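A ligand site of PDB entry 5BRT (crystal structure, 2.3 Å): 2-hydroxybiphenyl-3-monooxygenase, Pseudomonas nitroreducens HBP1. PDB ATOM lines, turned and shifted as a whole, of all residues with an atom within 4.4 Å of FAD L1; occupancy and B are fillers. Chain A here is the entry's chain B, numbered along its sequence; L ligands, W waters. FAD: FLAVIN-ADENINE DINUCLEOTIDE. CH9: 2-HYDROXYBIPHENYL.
OE1 of Gln 120 sits at hydrogen-bond distance from N of Ser 47 (2.9 Å). The side-chain amide nitrogen of Gln 120 sits at hydrogen-bond distance from the side-chain carboxylate of Glu 124 (2.8 Å). The side-chain amide oxygen (OD1) of Asn 36 is in hydrogen-bond range of the backbone NH (N) of Trp 38 (3.2 Å). The backbone carbonyl oxygen (O) of Asn 36 is in hydrogen-bond range of the backbone NH (N) of Thr 142 (2.8 Å). The backbone NH of Gly 13 lies within hydrogen-bond range of the backbone carbonyl oxygen of Ile 35 (2.9 Å). The backbone NH (N) of Asp 178 lies within hydrogen-bond range of the backbone carbonyl oxygen (O) of Val 12, at 3.0 Å. The backbone NH (N) of Ala 177 sits at hydrogen-bond distance from the backbone carbonyl oxygen (O) of Val 12 (2.9 Å). NH2 of Arg 242 lies within hydrogen-bond range of O of Arg 46, 2.4 Å away.
Water W5 lies within hydrogen-bond range of OD2 of Asp 178 (2.7 Å) and N7A of FAD L1 (2.8 Å). Water W1 bridges OD2 of Asp 313 (2.8 Å) and O2A of FAD L1 (2.9 Å). Water W3 lies within hydrogen-bond range of NH1 of Arg 46 (2.6 Å), O2' of FAD L1 (2.9 Å) and NE2 of Gln 120 (3.3 Å). Water W6 lies within hydrogen-bond range of O of Ala 177 (2.7 Å), N of Gly 15 (2.9 Å) and O2P of FAD L1 (3.0 Å). Water W4 bridges OG of Ser 47 (3.2 Å) and O2 of FAD L1 (3.4 Å).
An oxygen (O2') of FAD L1 sits at hydrogen-bond distance from the side-chain amide oxygen (OE1) of Gln 120 (2.5 Å). The backbone NH (N) of Asp 313 is in hydrogen-bond range of an oxygen (O1P) of FAD L1 (2.6 Å). O3' of FAD L1 lies within hydrogen-bond range of OD1 of Asp 313 (2.5 Å). The side-chain amide oxygen (OD1) of Asn 36 is in hydrogen-bond range of an oxygen (O2B) of FAD L1 (2.7 Å). The backbone NH of Tyr 144 is in hydrogen-bond range of a nitrogen (N1A) of FAD L1 (2.9 Å). The backbone carbonyl oxygen (O) of Tyr 144 is in hydrogen-bond range of a nitrogen (N6A) of FAD L1 (3.2 Å). The indole nitrogen (NE1) of Trp 38 lies close to an oxygen (O2B) of FAD L1 (3.3 Å). N of Ala 17 is in hydrogen-bond range of O2P of FAD L1 (2.9 Å). The backbone NH of Arg 37 sits at hydrogen-bond distance from a nitrogen (N3A) of FAD L1, 3.2 Å away. N of Ala 14 is in hydrogen-bond range of O3B of FAD L1, at 3.4 Å.
N of Pro 16 sits close to O2P of FAD L1. CG1 of Val 12 touches N1A of FAD L1 (3.9 Å). Gly 13 touches FAD L1. Gly 15 touches FAD L1 (C to O2P, 3.4 Å). Arg 46 touches FAD L1. OG of Ser 47 touches O2 of FAD L1, 3.5 Å away. Thr 142 touches FAD L1 (O to C2A, 3.5 Å). Glu 143 touches FAD L1 (CA to N1A, 3.7 Å). O of Ala 177 touches C5B of FAD L1 (3.3 Å). O of Asp 178 touches C8A of FAD L1 (3.2 Å). Gly 179 touches FAD L1. Arg 242 touches FAD L1. Thr 292 touches FAD L1 (O to C7M, 3.9 Å). CZ2 of Trp 293 touches N10 of FAD L1, 3.3 Å away. Gly 312 touches FAD L1. Pro 320 touches FAD L1. CA of Gly 323 touches O2 of FAD L1, at 3.9 Å. Ser 329 touches FAD L1 (OG to O1P, 3.6 Å). Hydrophobic or aromatic side chains within 4 Å of FAD L1: Val 12, Pro 16, Ala 17, Trp 38, Tyr 144, Trp 293 and Pro 320. 26 residues have an atom within 4 Å of FAD L1: Val 12, Gly 13, Ala 14, Gly 15, Pro 16, Ala 17, Asn 36, Arg 37, Trp 38, Arg 46, Ser 47, Gln 120, Thr 142, Glu 143, Tyr 144, Ala 177, Asp 178, Gly 179, Arg 242, Thr 292, Trp 293, Gly 312, Asp 313, Pro 320, Gly 323 and Ser 329. The nearest printed residue that does not touch FAD L1 is Asn 205 (4.01 Å).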
ATOM      1  N   VAL A  12      25.485 -32.133  -9.135  1.00  0.00           N
ATOM      2  CA  VAL A  12      24.736 -31.824  -7.927  1.00  0.00           C
ATOM      3  C   VAL A  12      23.778 -30.709  -8.213  1.00  0.00           C
ATOM      4  O   VAL A  12      24.173 -29.560  -8.337  1.00  0.00           O
ATOM      5  CB  VAL A  12      25.642 -31.470  -6.726  1.00  0.00           C
ATOM      6  CG1 VAL A  12      24.789 -31.192  -5.489  1.00  0.00           C
ATOM      7  CG2 VAL A  12      26.622 -32.612  -6.461  1.00  0.00           C
ATOM      8  N   GLY A  13      22.500 -31.067  -8.360  1.00  0.00           N
ATOM      9  CA  GLY A  13      21.505 -30.094  -8.774  1.00  0.00           C
ATOM     10  C   GLY A  13      20.821 -30.466 -10.087  1.00  0.00           C
ATOM     11  O   GLY A  13      21.464 -30.881 -11.041  1.00  0.00           O
ATOM     12  N   ALA A  14      19.514 -30.305 -10.102  1.00  0.00           N
ATOM     13  CA  ALA A  14      18.709 -30.593 -11.275  1.00  0.00           C
ATOM     14  C   ALA A  14      17.923 -29.372 -11.731  1.00  0.00           C
ATOM     15  O   ALA A  14      16.873 -29.505 -12.360  1.00  0.00           O
ATOM     16  CB  ALA A  14      17.756 -31.775 -10.974  1.00  0.00           C
ATOM     17  N   GLY A  15      18.418 -28.184 -11.410  1.00  0.00           N
ATOM     18  CA  GLY A  15      17.848 -26.957 -11.944  1.00  0.00           C
ATOM     19  C   GLY A  15      18.268 -26.842 -13.394  1.00  0.00           C
ATOM     20  O   GLY A  15      18.854 -27.763 -13.936  1.00  0.00           O
ATOM     21  N   PRO A  16      18.019 -25.688 -14.020  1.00  0.00           N
ATOM     22  CA  PRO A  16      18.389 -25.448 -15.414  1.00  0.00           C
ATOM     23  C   PRO A  16      19.851 -25.812 -15.724  1.00  0.00           C
ATOM     24  O   PRO A  16      20.126 -26.489 -16.712  1.00  0.00           O
ATOM     25  CB  PRO A  16      18.178 -23.948 -15.574  1.00  0.00           C
ATOM     26  CG  PRO A  16      17.128 -23.624 -14.571  1.00  0.00           C
ATOM     27  CD  PRO A  16      17.393 -24.514 -13.401  1.00  0.00           C
ATOM     28  N   ALA A  17      20.799 -25.369 -14.891  1.00  0.00           N
ATOM     29  CA  ALA A  17      22.201 -25.691 -15.145  1.00  0.00           C
ATOM     30  C   ALA A  17      22.498 -27.202 -15.048  1.00  0.00           C
ATOM     31  O   ALA A  17      23.087 -27.801 -15.951  1.00  0.00           O
ATOM     32  CB  ALA A  17      23.113 -24.908 -14.200  1.00  0.00           C
ATOM     33  N   ILE A  35      21.683 -35.474  -9.308  1.00  0.00           N
ATOM     34  CA  ILE A  35      20.872 -35.576  -8.119  1.00  0.00           C
ATOM     35  C   ILE A  35      20.206 -34.261  -7.763  1.00  0.00           C
ATOM     36  O   ILE A  35      20.586 -33.190  -8.233  1.00  0.00           O
ATOM     37  CB  ILE A  35      21.650 -36.129  -6.909  1.00  0.00           C
ATOM     38  CG1 ILE A  35      22.726 -35.138  -6.459  1.00  0.00           C
ATOM     39  CG2 ILE A  35      22.243 -37.496  -7.244  1.00  0.00           C
ATOM     40  CD1 ILE A  35      23.394 -35.497  -5.129  1.00  0.00           C
ATOM     41  N   ASN A  36      19.160 -34.395  -6.956  1.00  0.00           N
ATOM     42  CA  ASN A  36      18.365 -33.270  -6.507  1.00  0.00           C
ATOM     43  C   ASN A  36      17.818 -33.640  -5.155  1.00  0.00           C
ATOM     44  O   ASN A  36      17.318 -34.756  -4.940  1.00  0.00           O
ATOM     45  CB  ASN A  36      17.207 -32.978  -7.477  1.00  0.00           C
ATOM     46  CG  ASN A  36      16.364 -31.764  -7.028  1.00  0.00           C
ATOM     47  OD1 ASN A  36      16.747 -31.018  -6.125  1.00  0.00           O
ATOM     48  ND2 ASN A  36      15.222 -31.568  -7.672  1.00  0.00           N
ATOM     49  N   ARG A  37      17.948 -32.699  -4.225  1.00  0.00           N
ATOM     50  CA  ARG A  37      17.528 -32.879  -2.853  1.00  0.00           C
ATOM     51  C   ARG A  37      16.023 -33.058  -2.760  1.00  0.00           C
ATOM     52  O   ARG A  37      15.541 -33.882  -1.979  1.00  0.00           O
ATOM     53  CB  ARG A  37      17.988 -31.664  -2.036  1.00  0.00           C
ATOM     54  CG  ARG A  37      17.184 -31.383  -0.786  1.00  0.00           C
ATOM     55  CD  ARG A  37      17.402 -32.468   0.250  1.00  0.00           C
ATOM     56  NE  ARG A  37      16.628 -32.254   1.473  1.00  0.00           N
ATOM     57  CZ  ARG A  37      15.367 -32.662   1.644  1.00  0.00           C
ATOM     58  NH1 ARG A  37      14.724 -33.285   0.663  1.00  0.00           N
ATOM     59  NH2 ARG A  37      14.746 -32.430   2.796  1.00  0.00           N
ATOM     60  N   TRP A  38      15.282 -32.298  -3.568  1.00  0.00           N
ATOM     61  CA  TRP A  38      13.837 -32.251  -3.441  1.00  0.00           C
ATOM     62  C   TRP A  38      13.102 -33.309  -4.272  1.00  0.00           C
ATOM     63  O   TRP A  38      13.696 -34.023  -5.069  1.00  0.00           O
ATOM     64  CB  TRP A  38      13.314 -30.846  -3.757  1.00  0.00           C
ATOM     65  CG  TRP A  38      14.052 -29.777  -2.990  1.00  0.00           C
ATOM     66  CD1 TRP A  38      14.893 -28.836  -3.502  1.00  0.00           C
ATOM     67  CD2 TRP A  38      14.040 -29.570  -1.569  1.00  0.00           C
ATOM     68  NE1 TRP A  38      15.391 -28.040  -2.493  1.00  0.00           N
ATOM     69  CE2 TRP A  38      14.886 -28.476  -1.304  1.00  0.00           C
ATOM     70  CE3 TRP A  38      13.378 -30.193  -0.506  1.00  0.00           C
ATOM     71  CZ2 TRP A  38      15.102 -27.997  -0.004  1.00  0.00           C
ATOM     72  CZ3 TRP A  38      13.593 -29.714   0.779  1.00  0.00           C
ATOM     73  CH2 TRP A  38      14.436 -28.632   1.023  1.00  0.00           C
ATOM     74  N   ARG A  46       9.194 -18.852 -11.163  1.00  0.00           N
ATOM     75  CA  ARG A  46      10.571 -18.347 -11.066  1.00  0.00           C
ATOM     76  C   ARG A  46      11.032 -17.671 -12.355  1.00  0.00           C
ATOM     77  O   ARG A  46      10.276 -16.877 -12.916  1.00  0.00           O
ATOM     78  CB  ARG A  46      11.533 -19.468 -10.631  1.00  0.00           C
ATOM     79  CG  ARG A  46      11.192 -20.006  -9.243  1.00  0.00           C
ATOM     80  CD  ARG A  46      12.098 -21.136  -8.794  1.00  0.00           C
ATOM     81  NE  ARG A  46      11.652 -21.643  -7.498  1.00  0.00           N
ATOM     82  CZ  ARG A  46      12.274 -22.605  -6.810  1.00  0.00           C
ATOM     83  NH1 ARG A  46      13.384 -23.171  -7.275  1.00  0.00           N
ATOM     84  NH2 ARG A  46      11.774 -23.000  -5.649  1.00  0.00           N
ATOM     85  N   SER A  47      12.236 -17.976 -12.821  1.00  0.00           N
ATOM     86  CA  SER A  47      12.724 -17.332 -14.039  1.00  0.00           C
ATOM     87  C   SER A  47      11.833 -17.720 -15.219  1.00  0.00           C
ATOM     88  O   SER A  47      11.368 -18.864 -15.314  1.00  0.00           O
ATOM     89  CB  SER A  47      14.166 -17.750 -14.321  1.00  0.00           C
ATOM     90  OG  SER A  47      14.658 -17.141 -15.497  1.00  0.00           O
ATOM     91  N   GLN A 120      10.127 -21.513 -15.482  1.00  0.00           N
ATOM     92  CA  GLN A 120      10.906 -22.648 -15.026  1.00  0.00           C
ATOM     93  C   GLN A 120      10.032 -23.847 -14.718  1.00  0.00           C
ATOM     94  O   GLN A 120      10.410 -24.987 -14.997  1.00  0.00           O
ATOM     95  CB  GLN A 120      11.713 -22.284 -13.768  1.00  0.00           C
ATOM     96  CG  GLN A 120      13.195 -22.125 -14.003  1.00  0.00           C
ATOM     97  CD  GLN A 120      13.929 -21.518 -12.824  1.00  0.00           C
ATOM     98  OE1 GLN A 120      13.971 -20.303 -12.658  1.00  0.00           O
ATOM     99  NE2 GLN A 120      14.499 -22.384 -11.987  1.00  0.00           N
ATOM    100  N   GLU A 124      11.951 -26.792 -16.653  1.00  0.00           N
ATOM    101  CA  GLU A 124      12.743 -27.768 -15.901  1.00  0.00           C
ATOM    102  C   GLU A 124      12.384 -29.212 -16.193  1.00  0.00           C
ATOM    103  O   GLU A 124      13.246 -30.012 -16.537  1.00  0.00           O
ATOM    104  CB  GLU A 124      12.716 -27.482 -14.381  1.00  0.00           C
ATOM    105  CG  GLU A 124      13.534 -26.291 -13.968  1.00  0.00           C
ATOM    106  CD  GLU A 124      13.691 -26.193 -12.469  1.00  0.00           C
ATOM    107  OE1 GLU A 124      13.398 -27.181 -11.766  1.00  0.00           O
ATOM    108  OE2 GLU A 124      14.121 -25.131 -11.992  1.00  0.00           O
ATOM    109  N   THR A 142      17.568 -36.891  -3.116  1.00  0.00           N
ATOM    110  CA  THR A 142      18.917 -37.367  -2.831  1.00  0.00           C
ATOM    111  C   THR A 142      19.794 -36.154  -2.609  1.00  0.00           C
ATOM    112  O   THR A 142      19.866 -35.259  -3.468  1.00  0.00           O
ATOM    113  CB  THR A 142      19.442 -38.249  -3.967  1.00  0.00           C
ATOM    114  OG1 THR A 142      18.503 -39.310  -4.204  1.00  0.00           O
ATOM    115  CG2 THR A 142      20.782 -38.870  -3.576  1.00  0.00           C
ATOM    116  N   GLU A 143      20.440 -36.128  -1.450  1.00  0.00           N
ATOM    117  CA  GLU A 143      21.113 -34.920  -0.973  1.00  0.00           C
ATOM    118  C   GLU A 143      22.621 -35.088  -0.923  1.00  0.00           C
ATOM    119  O   GLU A 143      23.154 -36.004  -0.298  1.00  0.00           O
ATOM    120  CB  GLU A 143      20.605 -34.556   0.419  1.00  0.00           C
ATOM    121  CG  GLU A 143      21.240 -33.287   0.981  1.00  0.00           C
ATOM    122  CD  GLU A 143      20.675 -32.917   2.330  1.00  0.00           C
ATOM    123  OE1 GLU A 143      20.012 -33.791   2.948  1.00  0.00           O
ATOM    124  OE2 GLU A 143      20.902 -31.768   2.765  1.00  0.00           O
ATOM    125  N   TYR A 144      23.321 -34.165  -1.583  1.00  0.00           N
ATOM    126  CA  TYR A 144      24.764 -34.130  -1.492  1.00  0.00           C
ATOM    127  C   TYR A 144      25.142 -33.626  -0.108  1.00  0.00           C
ATOM    128  O   TYR A 144      24.634 -32.611   0.356  1.00  0.00           O
ATOM    129  CB  TYR A 144      25.318 -33.237  -2.605  1.00  0.00           C
ATOM    130  CG  TYR A 144      26.719 -32.730  -2.352  1.00  0.00           C
ATOM    131  CD1 TYR A 144      27.833 -33.488  -2.739  1.00  0.00           C
ATOM    132  CD2 TYR A 144      26.932 -31.501  -1.762  1.00  0.00           C
ATOM    133  CE1 TYR A 144      29.118 -33.013  -2.521  1.00  0.00           C
ATOM    134  CE2 TYR A 144      28.193 -31.028  -1.545  1.00  0.00           C
ATOM    135  CZ  TYR A 144      29.277 -31.782  -1.924  1.00  0.00           C
ATOM    136  OH  TYR A 144      30.527 -31.281  -1.707  1.00  0.00           O
ATOM    137  N   ALA A 177      26.015 -27.713  -9.503  1.00  0.00           N
ATOM    138  CA  ALA A 177      24.904 -26.946 -10.057  1.00  0.00           C
ATOM    139  C   ALA A 177      23.832 -26.797  -9.004  1.00  0.00           C
ATOM    140  O   ALA A 177      22.642 -26.871  -9.300  1.00  0.00           O
ATOM    141  CB  ALA A 177      24.341 -27.633 -11.306  1.00  0.00           C
ATOM    142  N   ASP A 178      24.255 -26.597  -7.753  1.00  0.00           N
ATOM    143  CA  ASP A 178      23.382 -26.687  -6.614  1.00  0.00           C
ATOM    144  C   ASP A 178      22.926 -25.343  -6.060  1.00  0.00           C
ATOM    145  O   ASP A 178      22.590 -25.233  -4.872  1.00  0.00           O
ATOM    146  CB  ASP A 178      24.032 -27.540  -5.522  1.00  0.00           C
ATOM    147  CG  ASP A 178      25.389 -27.042  -5.121  1.00  0.00           C
ATOM    148  OD1 ASP A 178      26.019 -26.317  -5.944  1.00  0.00           O
ATOM    149  OD2 ASP A 178      25.824 -27.357  -3.989  1.00  0.00           O
ATOM    150  N   GLY A 179      22.942 -24.319  -6.897  1.00  0.00           N
ATOM    151  CA  GLY A 179      22.190 -23.122  -6.604  1.00  0.00           C
ATOM    152  C   GLY A 179      22.854 -22.104  -5.702  1.00  0.00           C
ATOM    153  O   GLY A 179      24.024 -22.241  -5.327  1.00  0.00           O
ATOM    154  N   ASN A 205       6.637 -13.392  -3.572  1.00  0.00           N
ATOM    155  CA  ASN A 205       5.991 -13.778  -4.808  1.00  0.00           C
ATOM    156  C   ASN A 205       4.653 -14.452  -4.508  1.00  0.00           C
ATOM    157  O   ASN A 205       4.604 -15.467  -3.812  1.00  0.00           O
ATOM    158  CB  ASN A 205       6.925 -14.696  -5.611  1.00  0.00           C
ATOM    159  CG  ASN A 205       8.180 -13.954  -6.130  1.00  0.00           C
ATOM    160  OD1 ASN A 205       8.368 -12.773  -5.858  1.00  0.00           O
ATOM    161  ND2 ASN A 205       9.019 -14.665  -6.870  1.00  0.00           N
ATOM    162  N   ARG A 242       3.126 -10.061 -13.121  1.00  0.00           N
ATOM    163  CA  ARG A 242       3.803 -10.798 -14.186  1.00  0.00           C
ATOM    164  C   ARG A 242       2.946 -11.957 -14.677  1.00  0.00           C
ATOM    165  O   ARG A 242       2.376 -12.707 -13.883  1.00  0.00           O
ATOM    166  CB  ARG A 242       5.155 -11.307 -13.676  1.00  0.00           C
ATOM    167  CG  ARG A 242       5.708 -12.534 -14.386  1.00  0.00           C
ATOM    168  CD  ARG A 242       6.784 -13.180 -13.536  1.00  0.00           C
ATOM    169  NE  ARG A 242       7.070 -14.554 -13.948  1.00  0.00           N
ATOM    170  CZ  ARG A 242       7.771 -15.422 -13.224  1.00  0.00           C
ATOM    171  NH1 ARG A 242       8.251 -15.073 -12.038  1.00  0.00           N
ATOM    172  NH2 ARG A 242       7.984 -16.646 -13.687  1.00  0.00           N
ATOM    173  N   THR A 292       8.914 -16.438  -0.804  1.00  0.00           N
ATOM    174  CA  THR A 292       9.897 -15.368  -0.758  1.00  0.00           C
ATOM    175  C   THR A 292      11.164 -15.796  -1.486  1.00  0.00           C
ATOM    176  O   THR A 292      11.403 -16.988  -1.701  1.00  0.00           O
ATOM    177  CB  THR A 292      10.231 -14.983   0.690  1.00  0.00           C
ATOM    178  OG1 THR A 292      11.097 -15.972   1.259  1.00  0.00           O
ATOM    179  CG2 THR A 292       8.971 -14.891   1.524  1.00  0.00           C
ATOM    180  N   TRP A 293      11.961 -14.818  -1.871  1.00  0.00           N
ATOM    181  CA  TRP A 293      13.209 -15.050  -2.577  1.00  0.00           C
ATOM    182  C   TRP A 293      14.203 -14.024  -2.064  1.00  0.00           C
ATOM    183  O   TRP A 293      14.025 -12.829  -2.294  1.00  0.00           O
ATOM    184  CB  TRP A 293      12.992 -14.858  -4.084  1.00  0.00           C
ATOM    185  CG  TRP A 293      14.224 -15.103  -4.946  1.00  0.00           C
ATOM    186  CD1 TRP A 293      15.274 -15.939  -4.675  1.00  0.00           C
ATOM    187  CD2 TRP A 293      14.526 -14.486  -6.207  1.00  0.00           C
ATOM    188  NE1 TRP A 293      16.198 -15.880  -5.686  1.00  0.00           N
ATOM    189  CE2 TRP A 293      15.763 -15.002  -6.644  1.00  0.00           C
ATOM    190  CE3 TRP A 293      13.868 -13.546  -7.016  1.00  0.00           C
ATOM    191  CZ2 TRP A 293      16.358 -14.611  -7.840  1.00  0.00           C
ATOM    192  CZ3 TRP A 293      14.460 -13.166  -8.205  1.00  0.00           C
ATOM    193  CH2 TRP A 293      15.694 -13.694  -8.606  1.00  0.00           C
ATOM    194  N   MET A 311      28.552 -23.970 -11.488  1.00  0.00           N
ATOM    195  CA  MET A 311      27.861 -23.288 -12.572  1.00  0.00           C
ATOM    196  C   MET A 311      26.513 -22.810 -12.093  1.00  0.00           C
ATOM    197  O   MET A 311      26.033 -23.262 -11.045  1.00  0.00           O
ATOM    198  CB  MET A 311      27.680 -24.245 -13.750  1.00  0.00           C
ATOM    199  CG  MET A 311      26.983 -25.562 -13.364  1.00  0.00           C
ATOM    200  SD  MET A 311      26.402 -26.447 -14.825  1.00  0.00           S
ATOM    201  CE  MET A 311      27.963 -27.008 -15.530  1.00  0.00           C
ATOM    202  N   GLY A 312      25.872 -21.919 -12.852  1.00  0.00           N
ATOM    203  CA  GLY A 312      24.536 -21.458 -12.493  1.00  0.00           C
ATOM    204  C   GLY A 312      24.579 -20.507 -11.301  1.00  0.00           C
ATOM    205  O   GLY A 312      25.584 -19.806 -11.098  1.00  0.00           O
ATOM    206  N   ASP A 313      23.492 -20.481 -10.530  1.00  0.00           N
ATOM    207  CA  ASP A 313      23.378 -19.670  -9.316  1.00  0.00           C
ATOM    208  C   ASP A 313      24.500 -19.965  -8.326  1.00  0.00           C
ATOM    209  O   ASP A 313      24.778 -19.140  -7.480  1.00  0.00           O
ATOM    210  CB  ASP A 313      22.043 -19.926  -8.601  1.00  0.00           C
ATOM    211  CG  ASP A 313      20.928 -18.997  -9.085  1.00  0.00           C
ATOM    212  OD1 ASP A 313      21.086 -18.316 -10.134  1.00  0.00           O
ATOM    213  OD2 ASP A 313      19.865 -18.971  -8.427  1.00  0.00           O
ATOM    214  N   PRO A 320      16.754 -10.226 -10.520  1.00  0.00           N
ATOM    215  CA  PRO A 320      16.124 -10.756 -11.734  1.00  0.00           C
ATOM    216  C   PRO A 320      16.161  -9.789 -12.925  1.00  0.00           C
ATOM    217  O   PRO A 320      15.799 -10.187 -14.041  1.00  0.00           O
ATOM    218  CB  PRO A 320      14.681 -10.992 -11.302  1.00  0.00           C
ATOM    219  CG  PRO A 320      14.465 -10.073 -10.166  1.00  0.00           C
ATOM    220  CD  PRO A 320      15.779  -9.959  -9.453  1.00  0.00           C
ATOM    221  N   GLY A 323      16.494 -10.794 -16.670  1.00  0.00           N
ATOM    222  CA  GLY A 323      16.277 -12.220 -16.870  1.00  0.00           C
ATOM    223  C   GLY A 323      17.520 -12.961 -17.328  1.00  0.00           C
ATOM    224  O   GLY A 323      17.457 -13.809 -18.216  1.00  0.00           O
ATOM    225  N   GLY A 325      19.637 -14.789 -15.335  1.00  0.00           N
ATOM    226  CA  GLY A 325      19.987 -15.922 -14.476  1.00  0.00           C
ATOM    227  C   GLY A 325      19.944 -17.277 -15.143  1.00  0.00           C
ATOM    228  O   GLY A 325      20.976 -17.936 -15.360  1.00  0.00           O
ATOM    229  N   LEU A 326      18.730 -17.712 -15.474  1.00  0.00           N
ATOM    230  CA  LEU A 326      18.539 -19.015 -16.050  1.00  0.00           C
ATOM    231  C   LEU A 326      19.328 -19.152 -17.336  1.00  0.00           C
ATOM    232  O   LEU A 326      19.989 -20.148 -17.559  1.00  0.00           O
ATOM    233  CB  LEU A 326      17.052 -19.262 -16.317  1.00  0.00           C
ATOM    234  CG  LEU A 326      16.763 -20.620 -16.928  1.00  0.00           C
ATOM    235  CD1 LEU A 326      15.445 -21.129 -16.403  1.00  0.00           C
ATOM    236  CD2 LEU A 326      16.706 -20.525 -18.456  1.00  0.00           C
ATOM    237  N   SER A 329      22.993 -19.499 -16.784  1.00  0.00           N
ATOM    238  CA  SER A 329      23.196 -20.801 -16.158  1.00  0.00           C
ATOM    239  C   SER A 329      23.211 -21.915 -17.186  1.00  0.00           C
ATOM    240  O   SER A 329      24.049 -22.809 -17.120  1.00  0.00           O
ATOM    241  CB  SER A 329      22.114 -21.047 -15.117  1.00  0.00           C
ATOM    242  OG  SER A 329      22.227 -20.102 -14.074  1.00  0.00           O
HETATM  243  PA  FAD L   1      18.694 -23.967  -9.161  1.00  0.00           P
HETATM  244  O1A FAD L   1      17.486 -23.772 -10.116  1.00  0.00           O
HETATM  245  O2A FAD L   1      18.382 -23.293  -7.812  1.00  0.00           O
HETATM  246  O5B FAD L   1      19.037 -25.486  -8.986  1.00  0.00           O
HETATM  247  C5B FAD L   1      19.778 -25.932  -7.882  1.00  0.00           C
HETATM  248  C4B FAD L   1      19.449 -27.394  -7.686  1.00  0.00           C
HETATM  249  O4B FAD L   1      20.299 -28.082  -6.807  1.00  0.00           O
HETATM  250  C3B FAD L   1      18.064 -27.591  -7.176  1.00  0.00           C
HETATM  251  O3B FAD L   1      17.570 -28.733  -7.759  1.00  0.00           O
HETATM  252  C2B FAD L   1      18.291 -27.811  -5.726  1.00  0.00           C
HETATM  253  O2B FAD L   1      17.267 -28.517  -5.172  1.00  0.00           O
HETATM  254  C1B FAD L   1      19.509 -28.646  -5.801  1.00  0.00           C
HETATM  255  N9A FAD L   1      20.326 -28.716  -4.627  1.00  0.00           N
HETATM  256  C8A FAD L   1      20.778 -27.710  -3.838  1.00  0.00           C
HETATM  257  N7A FAD L   1      21.540 -28.213  -2.889  1.00  0.00           N
HETATM  258  C5A FAD L   1      21.625 -29.533  -3.034  1.00  0.00           C
HETATM  259  C6A FAD L   1      22.246 -30.570  -2.359  1.00  0.00           C
HETATM  260  N6A FAD L   1      23.056 -30.304  -1.207  1.00  0.00           N
HETATM  261  N1A FAD L   1      22.106 -31.839  -2.786  1.00  0.00           N
HETATM  262  C2A FAD L   1      21.353 -32.158  -3.860  1.00  0.00           C
HETATM  263  N3A FAD L   1      20.720 -31.169  -4.549  1.00  0.00           N
HETATM  264  C4A FAD L   1      20.834 -29.884  -4.150  1.00  0.00           C
HETATM  265  N1  FAD L   1      15.226 -15.577 -11.705  1.00  0.00           N
HETATM  266  C2  FAD L   1      14.697 -14.603 -12.655  1.00  0.00           C
HETATM  267  O2  FAD L   1      15.367 -14.240 -13.611  1.00  0.00           O
HETATM  268  N3  FAD L   1      13.415 -14.051 -12.487  1.00  0.00           N
HETATM  269  C4  FAD L   1      12.613 -14.414 -11.418  1.00  0.00           C
HETATM  270  O4  FAD L   1      11.516 -13.910 -11.278  1.00  0.00           O
HETATM  271  C4X FAD L   1      13.115 -15.401 -10.446  1.00  0.00           C
HETATM  272  N5  FAD L   1      12.371 -15.770  -9.405  1.00  0.00           N
HETATM  273  C5X FAD L   1      12.909 -16.755  -8.441  1.00  0.00           C
HETATM  274  C6  FAD L   1      12.130 -17.144  -7.350  1.00  0.00           C
HETATM  275  C7  FAD L   1      12.606 -18.070  -6.428  1.00  0.00           C
HETATM  276  C7M FAD L   1      11.746 -18.472  -5.267  1.00  0.00           C
HETATM  277  C8  FAD L   1      13.875 -18.623  -6.589  1.00  0.00           C
HETATM  278  C8M FAD L   1      14.389 -19.610  -5.596  1.00  0.00           C
HETATM  279  C9  FAD L   1      14.676 -18.244  -7.672  1.00  0.00           C
HETATM  280  C9A FAD L   1      14.203 -17.306  -8.602  1.00  0.00           C
HETATM  281  N10 FAD L   1      14.973 -16.906  -9.720  1.00  0.00           N
HETATM  282  C10 FAD L   1      14.500 -15.968 -10.650  1.00  0.00           C
HETATM  283  C1' FAD L   1      16.292 -17.473  -9.881  1.00  0.00           C
HETATM  284  C2' FAD L   1      16.312 -18.639 -11.009  1.00  0.00           C
HETATM  285  O2' FAD L   1      15.386 -19.761 -10.708  1.00  0.00           O
HETATM  286  C3' FAD L   1      17.752 -19.041 -11.630  1.00  0.00           C
HETATM  287  O3' FAD L   1      18.769 -18.337 -11.038  1.00  0.00           O
HETATM  288  C4' FAD L   1      18.097 -20.531 -11.802  1.00  0.00           C
HETATM  289  O4' FAD L   1      17.069 -21.388 -11.431  1.00  0.00           O
HETATM  290  C5' FAD L   1      19.410 -21.009 -11.200  1.00  0.00           C
HETATM  291  O5' FAD L   1      19.740 -22.218 -11.811  1.00  0.00           O
HETATM  292  P   FAD L   1      20.652 -23.324 -11.136  1.00  0.00           P
HETATM  293  O1P FAD L   1      21.872 -22.398 -11.337  1.00  0.00           O
HETATM  294  O2P FAD L   1      20.139 -24.180 -12.307  1.00  0.00           O
HETATM  295  O3P FAD L   1      19.878 -23.109  -9.757  1.00  0.00           O
HETATM  296  CAH CH9 L   2      12.128  -8.011 -11.262  1.00  0.00           C
HETATM  297  CAC CH9 L   2      11.666  -7.812  -9.855  1.00  0.00           C
HETATM  298  CAB CH9 L   2      10.469  -8.312  -9.457  1.00  0.00           C
HETATM  299  CAD CH9 L   2       9.615  -9.056 -10.424  1.00  0.00           C
HETATM  300  CAI CH9 L   2      10.039  -9.240 -11.710  1.00  0.00           C
HETATM  301  CAL CH9 L   2      11.360  -8.701 -12.158  1.00  0.00           C
HETATM  302  CAM CH9 L   2      11.857  -8.880 -13.543  1.00  0.00           C
HETATM  303  CAJ CH9 L   2      12.664  -7.913 -14.069  1.00  0.00           C
HETATM  304  CAF CH9 L   2      13.201  -8.031 -15.448  1.00  0.00           C
HETATM  305  CAE CH9 L   2      12.873  -9.108 -16.215  1.00  0.00           C
HETATM  306  CAG CH9 L   2      12.000 -10.167 -15.660  1.00  0.00           C
HETATM  307  CAK CH9 L   2      11.510 -10.075 -14.388  1.00  0.00           C
HETATM  308  OAA CH9 L   2      10.702 -11.071 -13.911  1.00  0.00           O
HETATM  309  O   HOH W   1      19.444 -21.002  -6.490  1.00  0.00           O
HETATM  310  O   HOH W   2      23.737 -23.580  -9.438  1.00  0.00           O
HETATM  311  O   HOH W   3      15.158 -22.009  -8.820  1.00  0.00           O
HETATM  312  O   HOH W   4      13.247 -14.314 -16.234  1.00  0.00           O
HETATM  313  O   HOH W   5      24.071 -27.341  -1.938  1.00  0.00           O
HETATM  314  O   HOH W   6      21.049 -26.936 -11.449  1.00  0.00           O
